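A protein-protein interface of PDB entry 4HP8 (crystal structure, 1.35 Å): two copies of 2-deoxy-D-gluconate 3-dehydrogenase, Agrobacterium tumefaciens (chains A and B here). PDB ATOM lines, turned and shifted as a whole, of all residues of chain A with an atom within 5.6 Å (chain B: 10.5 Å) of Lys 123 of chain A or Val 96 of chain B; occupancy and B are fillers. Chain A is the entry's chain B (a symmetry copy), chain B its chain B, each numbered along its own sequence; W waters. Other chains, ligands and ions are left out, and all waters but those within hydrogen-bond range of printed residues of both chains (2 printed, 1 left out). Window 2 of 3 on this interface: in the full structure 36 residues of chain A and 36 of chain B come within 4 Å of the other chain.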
ATOM      1  N   THR A 118     -14.839 -26.749 -21.330  1.00  0.00           N
ATOM      2  CA  THR A 118     -15.887 -27.785 -21.327  1.00  0.00           C
ATOM      3  C   THR A 118     -16.983 -27.472 -22.330  1.00  0.00           C
ATOM      4  O   THR A 118     -17.453 -28.398 -23.008  1.00  0.00           O
ATOM      5  CB  THR A 118     -16.472 -27.946 -19.933  1.00  0.00           C
ATOM      6  OG1 THR A 118     -15.398 -28.190 -19.005  1.00  0.00           O
ATOM      7  CG2 THR A 118     -17.425 -29.106 -19.890  1.00  0.00           C
ATOM      8  N   GLN A 119     -17.377 -26.216 -22.460  1.00  0.00           N
ATOM      9  CA  GLN A 119     -18.386 -25.827 -23.425  1.00  0.00           C
ATOM     10  C   GLN A 119     -17.983 -26.211 -24.838  1.00  0.00           C
ATOM     11  O   GLN A 119     -18.803 -26.785 -25.578  1.00  0.00           O
ATOM     12  CB  GLN A 119     -18.594 -24.344 -23.333  1.00  0.00           C
ATOM     13  CG  GLN A 119     -19.659 -23.848 -24.314  1.00  0.00           C
ATOM     14  CD  GLN A 119     -19.752 -22.330 -24.292  1.00  0.00           C
ATOM     15  OE1 GLN A 119     -18.840 -21.641 -24.771  1.00  0.00           O
ATOM     16  NE2 GLN A 119     -20.844 -21.792 -23.731  1.00  0.00           N
ATOM     17  N   ALA A 120     -16.761 -25.904 -25.239  1.00  0.00           N
ATOM     18  CA  ALA A 120     -16.303 -26.227 -26.576  1.00  0.00           C
ATOM     19  C   ALA A 120     -16.227 -27.742 -26.785  1.00  0.00           C
ATOM     20  O   ALA A 120     -16.584 -28.230 -27.876  1.00  0.00           O
ATOM     21  CB  ALA A 120     -14.972 -25.541 -26.832  1.00  0.00           C
ATOM     22  N   PHE A 121     -15.734 -28.464 -25.791  1.00  0.00           N
ATOM     23  CA  PHE A 121     -15.695 -29.935 -25.888  1.00  0.00           C
ATOM     24  C   PHE A 121     -17.069 -30.535 -26.083  1.00  0.00           C
ATOM     25  O   PHE A 121     -17.282 -31.391 -26.976  1.00  0.00           O
ATOM     26  CB  PHE A 121     -15.024 -30.440 -24.612  1.00  0.00           C
ATOM     27  CG  PHE A 121     -15.132 -31.940 -24.351  1.00  0.00           C
ATOM     28  CD1 PHE A 121     -14.253 -32.854 -24.999  1.00  0.00           C
ATOM     29  CD2 PHE A 121     -16.086 -32.428 -23.454  1.00  0.00           C
ATOM     30  CE1 PHE A 121     -14.318 -34.225 -24.745  1.00  0.00           C
ATOM     31  CE2 PHE A 121     -16.166 -33.786 -23.209  1.00  0.00           C
ATOM     32  CZ  PHE A 121     -15.281 -34.686 -23.822  1.00  0.00           C
ATOM     33  N   ALA A 122     -18.011 -30.098 -25.257  1.00  0.00           N
ATOM     34  CA  ALA A 122     -19.376 -30.630 -25.360  1.00  0.00           C
ATOM     35  C   ALA A 122     -20.080 -30.181 -26.621  1.00  0.00           C
ATOM     36  O   ALA A 122     -20.923 -30.941 -27.128  1.00  0.00           O
ATOM     37  CB  ALA A 122     -20.187 -30.206 -24.124  1.00  0.00           C
ATOM     38  N   LYS A 123     -19.802 -28.969 -27.131  1.00  0.00           N
ATOM     39  CA  LYS A 123     -20.475 -28.496 -28.334  1.00  0.00           C
ATOM     40  C   LYS A 123     -20.221 -29.518 -29.419  1.00  0.00           C
ATOM     41  O   LYS A 123     -21.139 -29.833 -30.237  1.00  0.00           O
ATOM     42  CB  LYS A 123     -19.935 -27.119 -28.696  1.00  0.00           C
ATOM     43  CG  LYS A 123     -20.615 -26.554 -29.952  1.00  0.00           C
ATOM     44  CD  LYS A 123     -20.135 -25.141 -30.182  1.00  0.00           C
ATOM     45  CE  LYS A 123     -20.507 -24.674 -31.580  1.00  0.00           C
ATOM     46  NZ  LYS A 123     -21.016 -23.281 -31.514  1.00  0.00           N
ATOM     47  N   GLU A 124     -18.978 -29.968 -29.517  1.00  0.00           N
ATOM     48  CA  GLU A 124     -18.642 -30.914 -30.581  1.00  0.00           C
ATOM     49  C   GLU A 124     -19.351 -32.253 -30.411  1.00  0.00           C
ATOM     50  O   GLU A 124     -19.880 -32.819 -31.371  1.00  0.00           O
ATOM     51  CB  GLU A 124     -17.117 -31.117 -30.571  1.00  0.00           C
ATOM     52  CG  GLU A 124     -16.637 -32.164 -31.595  1.00  0.00           C
ATOM     53  CD  GLU A 124     -16.649 -31.688 -33.062  1.00  0.00           C
ATOM     54  OE1 GLU A 124     -17.054 -30.543 -33.362  1.00  0.00           O
ATOM     55  OE2 GLU A 124     -16.163 -32.464 -33.907  1.00  0.00           O
ATOM     56  N   LEU A 125     -19.410 -32.756 -29.187  1.00  0.00           N
ATOM     57  CA  LEU A 125     -20.132 -34.004 -28.943  1.00  0.00           C
ATOM     58  C   LEU A 125     -21.621 -33.882 -29.204  1.00  0.00           C
ATOM     59  O   LEU A 125     -22.223 -34.760 -29.867  1.00  0.00           O
ATOM     60  CB  LEU A 125     -19.929 -34.484 -27.507  1.00  0.00           C
ATOM     61  CG  LEU A 125     -18.484 -34.817 -27.110  1.00  0.00           C
ATOM     62  CD1 LEU A 125     -18.474 -35.140 -25.580  1.00  0.00           C
ATOM     63  CD2 LEU A 125     -17.913 -35.950 -27.874  1.00  0.00           C
ATOM     64  N   LEU A 126     -22.215 -32.825 -28.682  1.00  0.00           N
ATOM     65  CA  LEU A 126     -23.648 -32.645 -28.809  1.00  0.00           C
ATOM     66  C   LEU A 126     -24.027 -32.458 -30.272  1.00  0.00           C
ATOM     67  O   LEU A 126     -25.080 -32.983 -30.724  1.00  0.00           O
ATOM     68  CB  LEU A 126     -24.113 -31.460 -27.961  1.00  0.00           C
ATOM     69  CG  LEU A 126     -23.999 -31.680 -26.457  1.00  0.00           C
ATOM     70  CD1 LEU A 126     -24.126 -30.334 -25.695  1.00  0.00           C
ATOM     71  CD2 LEU A 126     -25.050 -32.719 -25.973  1.00  0.00           C
ATOM     72  N   ALA A 127     -23.200 -31.767 -31.061  1.00  0.00           N
ATOM     73  CA  ALA A 127     -23.537 -31.496 -32.444  1.00  0.00           C
ATOM     74  C   ALA A 127     -23.580 -32.789 -33.227  1.00  0.00           C
ATOM     75  O   ALA A 127     -24.305 -32.888 -34.240  1.00  0.00           O
ATOM     76  CB  ALA A 127     -22.511 -30.584 -33.077  1.00  0.00           C
ATOM     77  N   LYS A 128     -22.801 -33.773 -32.827  1.00  0.00           N
ATOM     78  CA  LYS A 128     -22.646 -35.023 -33.565  1.00  0.00           C
ATOM     79  C   LYS A 128     -23.393 -36.190 -32.960  1.00  0.00           C
ATOM     80  O   LYS A 128     -23.416 -37.289 -33.529  1.00  0.00           O
ATOM     81  CB  LYS A 128     -21.153 -35.361 -33.762  1.00  0.00           C
ATOM     82  CG  LYS A 128     -20.489 -34.335 -34.717  1.00  0.00           C
ATOM     83  CD  LYS A 128     -19.010 -34.579 -34.982  1.00  0.00           C
ATOM     84  CE  LYS A 128     -18.514 -33.531 -35.991  1.00  0.00           C
ATOM     85  NZ  LYS A 128     -17.116 -33.776 -36.329  1.00  0.00           N
ATOM     86  N   GLU A 169     -27.766 -30.949 -17.119  1.00  0.00           N
ATOM     87  CA  GLU A 169     -28.160 -30.516 -18.445  1.00  0.00           C
ATOM     88  C   GLU A 169     -27.809 -31.527 -19.514  1.00  0.00           C
ATOM     89  O   GLU A 169     -28.531 -31.599 -20.525  1.00  0.00           O
ATOM     90  CB  GLU A 169     -27.471 -29.181 -18.757  1.00  0.00           C
ATOM     91  CG  GLU A 169     -28.168 -28.373 -19.859  1.00  0.00           C
ATOM     92  CD  GLU A 169     -27.729 -26.901 -19.876  1.00  0.00           C
ATOM     93  OE1 GLU A 169     -27.364 -26.317 -18.814  1.00  0.00           O
ATOM     94  OE2 GLU A 169     -27.792 -26.352 -20.971  1.00  0.00           O
ATOM     95  N   TRP A 170     -26.721 -32.296 -19.345  1.00  0.00           N
ATOM     96  CA  TRP A 170     -26.195 -33.131 -20.429  1.00  0.00           C
ATOM     97  C   TRP A 170     -26.225 -34.621 -20.143  1.00  0.00           C
ATOM     98  O   TRP A 170     -25.920 -35.412 -21.064  1.00  0.00           O
ATOM     99  CB  TRP A 170     -24.739 -32.738 -20.725  1.00  0.00           C
ATOM    100  CG  TRP A 170     -24.539 -31.325 -21.252  1.00  0.00           C
ATOM    101  CD1 TRP A 170     -25.443 -30.522 -21.858  1.00  0.00           C
ATOM    102  CD2 TRP A 170     -23.322 -30.594 -21.201  1.00  0.00           C
ATOM    103  NE1 TRP A 170     -24.863 -29.298 -22.206  1.00  0.00           N
ATOM    104  CE2 TRP A 170     -23.548 -29.349 -21.817  1.00  0.00           C
ATOM    105  CE3 TRP A 170     -22.042 -30.882 -20.705  1.00  0.00           C
ATOM    106  CZ2 TRP A 170     -22.525 -28.364 -21.905  1.00  0.00           C
ATOM    107  CZ3 TRP A 170     -21.036 -29.911 -20.814  1.00  0.00           C
ATOM    108  CH2 TRP A 170     -21.289 -28.684 -21.414  1.00  0.00           C
ATOM    109  N   ARG B  92     -29.923 -16.833 -18.208  1.00  0.00           N
ATOM    110  CA  ARG B  92     -30.323 -18.177 -18.600  1.00  0.00           C
ATOM    111  C   ARG B  92     -30.102 -18.358 -20.079  1.00  0.00           C
ATOM    112  O   ARG B  92     -30.605 -17.547 -20.882  1.00  0.00           O
ATOM    113  CB  ARG B  92     -31.792 -18.410 -18.330  1.00  0.00           C
ATOM    114  CG  ARG B  92     -32.209 -18.257 -16.948  1.00  0.00           C
ATOM    115  CD  ARG B  92     -33.657 -18.647 -16.709  1.00  0.00           C
ATOM    116  NE  ARG B  92     -34.131 -18.034 -15.473  1.00  0.00           N
ATOM    117  CZ  ARG B  92     -34.056 -18.589 -14.266  1.00  0.00           C
ATOM    118  NH1 ARG B  92     -33.542 -19.807 -14.101  1.00  0.00           N
ATOM    119  NH2 ARG B  92     -34.518 -17.919 -13.214  1.00  0.00           N
ATOM    120  N   ALA B  93     -29.405 -19.427 -20.450  1.00  0.00           N
ATOM    121  CA  ALA B  93     -29.223 -19.856 -21.857  1.00  0.00           C
ATOM    122  C   ALA B  93     -28.717 -21.284 -21.815  1.00  0.00           C
ATOM    123  O   ALA B  93     -28.119 -21.703 -20.813  1.00  0.00           O
ATOM    124  CB  ALA B  93     -28.192 -18.955 -22.517  1.00  0.00           C
ATOM    125  N   ASP B  94     -28.898 -22.045 -22.883  1.00  0.00           N
ATOM    126  CA  ASP B  94     -28.290 -23.372 -22.949  1.00  0.00           C
ATOM    127  C   ASP B  94     -26.802 -23.276 -22.662  1.00  0.00           C
ATOM    128  O   ASP B  94     -26.114 -22.390 -23.220  1.00  0.00           O
ATOM    129  CB  ASP B  94     -28.479 -23.984 -24.354  1.00  0.00           C
ATOM    130  CG  ASP B  94     -29.928 -24.263 -24.694  1.00  0.00           C
ATOM    131  OD1 ASP B  94     -30.790 -24.356 -23.794  1.00  0.00           O
ATOM    132  OD2 ASP B  94     -30.202 -24.493 -25.896  1.00  0.00           O
ATOM    133  N   SER B  95     -26.283 -24.174 -21.830  1.00  0.00           N
ATOM    134  CA  SER B  95     -24.885 -24.059 -21.451  1.00  0.00           C
ATOM    135  C   SER B  95     -23.959 -24.171 -22.626  1.00  0.00           C
ATOM    136  O   SER B  95     -22.891 -23.528 -22.630  1.00  0.00           O
ATOM    137  CB  SER B  95     -24.537 -25.087 -20.401  1.00  0.00           C
ATOM    138  OG  SER B  95     -25.139 -24.729 -19.155  1.00  0.00           O
ATOM    139  N   VAL B  96     -24.339 -24.928 -23.654  1.00  0.00           N
ATOM    140  CA  VAL B  96     -23.470 -25.102 -24.817  1.00  0.00           C
ATOM    141  C   VAL B  96     -23.306 -23.789 -25.611  1.00  0.00           C
ATOM    142  O   VAL B  96     -22.336 -23.622 -26.374  1.00  0.00           O
ATOM    143  CB  VAL B  96     -23.970 -26.280 -25.687  1.00  0.00           C
ATOM    144  CG1 VAL B  96     -25.237 -25.918 -26.418  1.00  0.00           C
ATOM    145  CG2 VAL B  96     -22.869 -26.723 -26.631  1.00  0.00           C
ATOM    146  N   GLU B  97     -24.247 -22.857 -25.422  1.00  0.00           N
ATOM    147  CA  GLU B  97     -24.271 -21.549 -26.120  1.00  0.00           C
ATOM    148  C   GLU B  97     -24.010 -20.343 -25.216  1.00  0.00           C
ATOM    149  O   GLU B  97     -23.969 -19.192 -25.691  1.00  0.00           O
ATOM    150  CB  GLU B  97     -25.641 -21.338 -26.816  1.00  0.00           C
ATOM    151  CG  GLU B  97     -25.956 -22.407 -27.857  1.00  0.00           C
ATOM    152  CD  GLU B  97     -25.001 -22.372 -29.063  1.00  0.00           C
ATOM    153  OE1 GLU B  97     -24.554 -21.268 -29.441  1.00  0.00           O
ATOM    154  OE2 GLU B  97     -24.698 -23.455 -29.642  1.00  0.00           O
ATOM    155  N   PHE B  98     -23.817 -20.581 -23.925  1.00  0.00           N
ATOM    156  CA  PHE B  98     -23.744 -19.513 -22.932  1.00  0.00           C
ATOM    157  C   PHE B  98     -22.626 -18.517 -23.267  1.00  0.00           C
ATOM    158  O   PHE B  98     -21.476 -18.923 -23.534  1.00  0.00           O
ATOM    159  CB  PHE B  98     -23.504 -20.159 -21.574  1.00  0.00           C
ATOM    160  CG  PHE B  98     -23.947 -19.336 -20.419  1.00  0.00           C
ATOM    161  CD1 PHE B  98     -25.287 -19.404 -19.992  1.00  0.00           C
ATOM    162  CD2 PHE B  98     -23.058 -18.516 -19.730  1.00  0.00           C
ATOM    163  CE1 PHE B  98     -25.710 -18.634 -18.924  1.00  0.00           C
ATOM    164  CE2 PHE B  98     -23.498 -17.760 -18.634  1.00  0.00           C
ATOM    165  CZ  PHE B  98     -24.785 -17.809 -18.237  1.00  0.00           C
ATOM    166  N   SER B  99     -22.944 -17.224 -23.242  1.00  0.00           N
ATOM    167  CA  SER B  99     -21.967 -16.238 -23.691  1.00  0.00           C
ATOM    168  C   SER B  99     -20.977 -15.779 -22.616  1.00  0.00           C
ATOM    169  O   SER B  99     -21.215 -15.895 -21.412  1.00  0.00           O
ATOM    170  CB  SER B  99     -22.706 -15.001 -24.214  1.00  0.00           C
ATOM    171  OG  SER B  99     -23.288 -14.291 -23.125  1.00  0.00           O
ATOM    172  N   GLU B 100     -19.829 -15.295 -23.059  1.00  0.00           N
ATOM    173  CA  GLU B 100     -18.895 -14.684 -22.150  1.00  0.00           C
ATOM    174  C   GLU B 100     -19.479 -13.516 -21.370  1.00  0.00           C
ATOM    175  O   GLU B 100     -19.170 -13.364 -20.186  1.00  0.00           O
ATOM    176  CB  GLU B 100     -17.621 -14.256 -22.887  1.00  0.00           C
ATOM    177  CG  GLU B 100     -16.490 -13.867 -21.901  1.00  0.00           C
ATOM    178  CD  GLU B 100     -15.231 -13.375 -22.579  1.00  0.00           C
ATOM    179  OE1 GLU B 100     -15.252 -13.076 -23.807  1.00  0.00           O
ATOM    180  OE2 GLU B 100     -14.193 -13.259 -21.919  1.00  0.00           O
ATOM    181  N   ILE B 147     -30.118 -25.891 -14.182  1.00  0.00           N
ATOM    182  CA  ILE B 147     -29.737 -26.052 -15.578  1.00  0.00           C
ATOM    183  C   ILE B 147     -29.748 -24.652 -16.222  1.00  0.00           C
ATOM    184  O   ILE B 147     -30.499 -23.755 -15.776  1.00  0.00           O
ATOM    185  CB  ILE B 147     -30.691 -27.004 -16.414  1.00  0.00           C
ATOM    186  CG1 ILE B 147     -32.143 -26.484 -16.367  1.00  0.00           C
ATOM    187  CG2 ILE B 147     -30.543 -28.487 -16.005  1.00  0.00           C
ATOM    188  CD1 ILE B 147     -33.074 -27.214 -17.382  1.00  0.00           C
ATOM    189  N   ARG B 148     -28.948 -24.466 -17.256  1.00  0.00           N
ATOM    190  CA  ARG B 148     -29.011 -23.250 -18.111  1.00  0.00           C
ATOM    191  C   ARG B 148     -28.602 -21.969 -17.419  1.00  0.00           C
ATOM    192  O   ARG B 148     -28.734 -20.891 -17.996  1.00  0.00           O
ATOM    193  CB  ARG B 148     -30.369 -23.096 -18.832  1.00  0.00           C
ATOM    194  CG  ARG B 148     -30.685 -24.304 -19.712  1.00  0.00           C
ATOM    195  CD  ARG B 148     -32.034 -24.135 -20.429  1.00  0.00           C
ATOM    196  NE  ARG B 148     -31.960 -23.151 -21.504  1.00  0.00           N
ATOM    197  CZ  ARG B 148     -32.611 -21.998 -21.509  1.00  0.00           C
ATOM    198  NH1 ARG B 148     -33.379 -21.656 -20.486  1.00  0.00           N
ATOM    199  NH2 ARG B 148     -32.492 -21.182 -22.546  1.00  0.00           N
ATOM    200  N   VAL B 149     -28.028 -22.094 -16.219  1.00  0.00           N
ATOM    201  CA  VAL B 149     -27.566 -20.922 -15.464  1.00  0.00           C
ATOM    202  C   VAL B 149     -26.148 -21.152 -14.942  1.00  0.00           C
ATOM    203  O   VAL B 149     -25.855 -20.921 -13.755  1.00  0.00           O
ATOM    204  CB  VAL B 149     -28.558 -20.524 -14.348  1.00  0.00           C
ATOM    205  CG1 VAL B 149     -29.919 -20.050 -14.938  1.00  0.00           C
ATOM    206  CG2 VAL B 149     -28.797 -21.662 -13.318  1.00  0.00           C
ATOM    207  N   PRO B 150     -25.205 -21.529 -15.812  1.00  0.00           N
ATOM    208  CA  PRO B 150     -23.893 -21.953 -15.286  1.00  0.00           C
ATOM    209  C   PRO B 150     -23.180 -20.861 -14.483  1.00  0.00           C
ATOM    210  O   PRO B 150     -22.591 -21.166 -13.437  1.00  0.00           O
ATOM    211  CB  PRO B 150     -23.091 -22.340 -16.564  1.00  0.00           C
ATOM    212  CG  PRO B 150     -23.882 -21.703 -17.709  1.00  0.00           C
ATOM    213  CD  PRO B 150     -25.314 -21.783 -17.272  1.00  0.00           C
ATOM    214  N   SER B 151     -23.204 -19.608 -14.907  1.00  0.00           N
ATOM    215  CA  SER B 151     -22.515 -18.600 -14.105  1.00  0.00           C
ATOM    216  C   SER B 151     -23.208 -18.360 -12.769  1.00  0.00           C
ATOM    217  O   SER B 151     -22.506 -18.089 -11.775  1.00  0.00           O
ATOM    218  CB  SER B 151     -22.291 -17.292 -14.908  1.00  0.00           C
ATOM    219  OG  SER B 151     -23.554 -16.763 -15.356  1.00  0.00           O
HETATM  220  O   HOH W   1     -30.166 -26.807 -22.360  1.00  0.00           O
HETATM  221  O   HOH W   2     -19.370 -18.927 -26.066  1.00  0.00           O
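N of Ala 93 of chain B lies within hydrogen-bond range of O of Arg 148 of chain B. The guanidinium group (NE) of Arg 148 of chain B lies within salt-bridge range of the side-chain carboxylate (OD1) of Asp 94 of chain B, 2.8 Å away.
Printed residues of chain A that touch a printed residue of chain B: Gln 119, Lys 123, Leu 126 and Glu 169. Of the 14 printed residues of chain B, 7 touch a printed residue of chain A. Printed residues of chain B that touch a printed residue of chain A: Asp 94, Ser 95, Val 96, Glu 97, Phe 98, Ile 147 and Arg 148. Among the printed residues, 10 pairs touch across the chains. Among the printed residues, no Asp or Glu carboxylate lies within 4 Å of a Lys or Arg side-chain nitrogen of the other chain.
Among the printed residues, merely in contact across the chains: Gln 119 of chain A with Val 96 of chain B (3.4 Å), Lys 123 of chain A with Val 96 of chain B (3.4 Å), Glu 169 of chain A with Asp 94 of chain B (3.6 Å), Gln 119 of chain A with Glu 97 of chain B (3.8 Å), Glu 169 of chain A with Ile 147 of chain B (3.9 Å) and Leu 126 of chain A with Val 96 of chain B (3.9 Å).
Val 96 of chain B touches three residues of chain A. No residue of chain B comes within 4 Å of Ala 122 of chain A. Of the printed residues of chain A, Asp 94 of chain B touches Glu 169 (3.6 Å). Printed residues of chain A within 4 Å of Ile 147 of chain B: Glu 169 (3.9 Å). Lys 128 of chain A touches none of the printed residues of chain B. The nearest residue of chain A that does not touch Val 96 of chain B is Trp 170 of chain A (4.3 Å). The nearest printed residue of chain A that does not touch Asp 94 of chain B is Gln 119 of chain A (5.3 Å).
The backbone carbonyl oxygen (O) of Ser 95 of chain B lies within hydrogen-bond range of the side-chain amide nitrogen (NE2) of Gln 119 of chain A, 2.9 Å away. The side-chain carboxylate (OE1) of Glu 169 of chain A sits at hydrogen-bond distance from the side-chain hydroxyl (OG) of Ser 95 of chain B. The side-chain amide nitrogen (NE2) of Gln 119 of chain A is in hydrogen-bond range of the backbone carbonyl oxygen (O) of Phe 98 of chain B (2.9 Å). N of Arg 148 of chain B sits at hydrogen-bond distance from OE1 of Glu 169 of chain A (2.9 Å).
Water W1 lies within hydrogen-bond range of the side-chain carboxylate (OE2) of Glu 169 of chain A (2.8 Å) and the side-chain carboxylate (OD1) of Asp 94 of chain B (2.9 Å). Water W2 lies within hydrogen-bond range of the side-chain amide oxygen (OE1) of Gln 119 of chain A (3.1 Å) and the backbone carbonyl oxygen (O) of Phe 98 of chain B (3.3 Å).
No position is printed for both chains. Of the 10 pairs that touch across the chains among the printed residues, none has its exchanged pair printed and touching as well.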
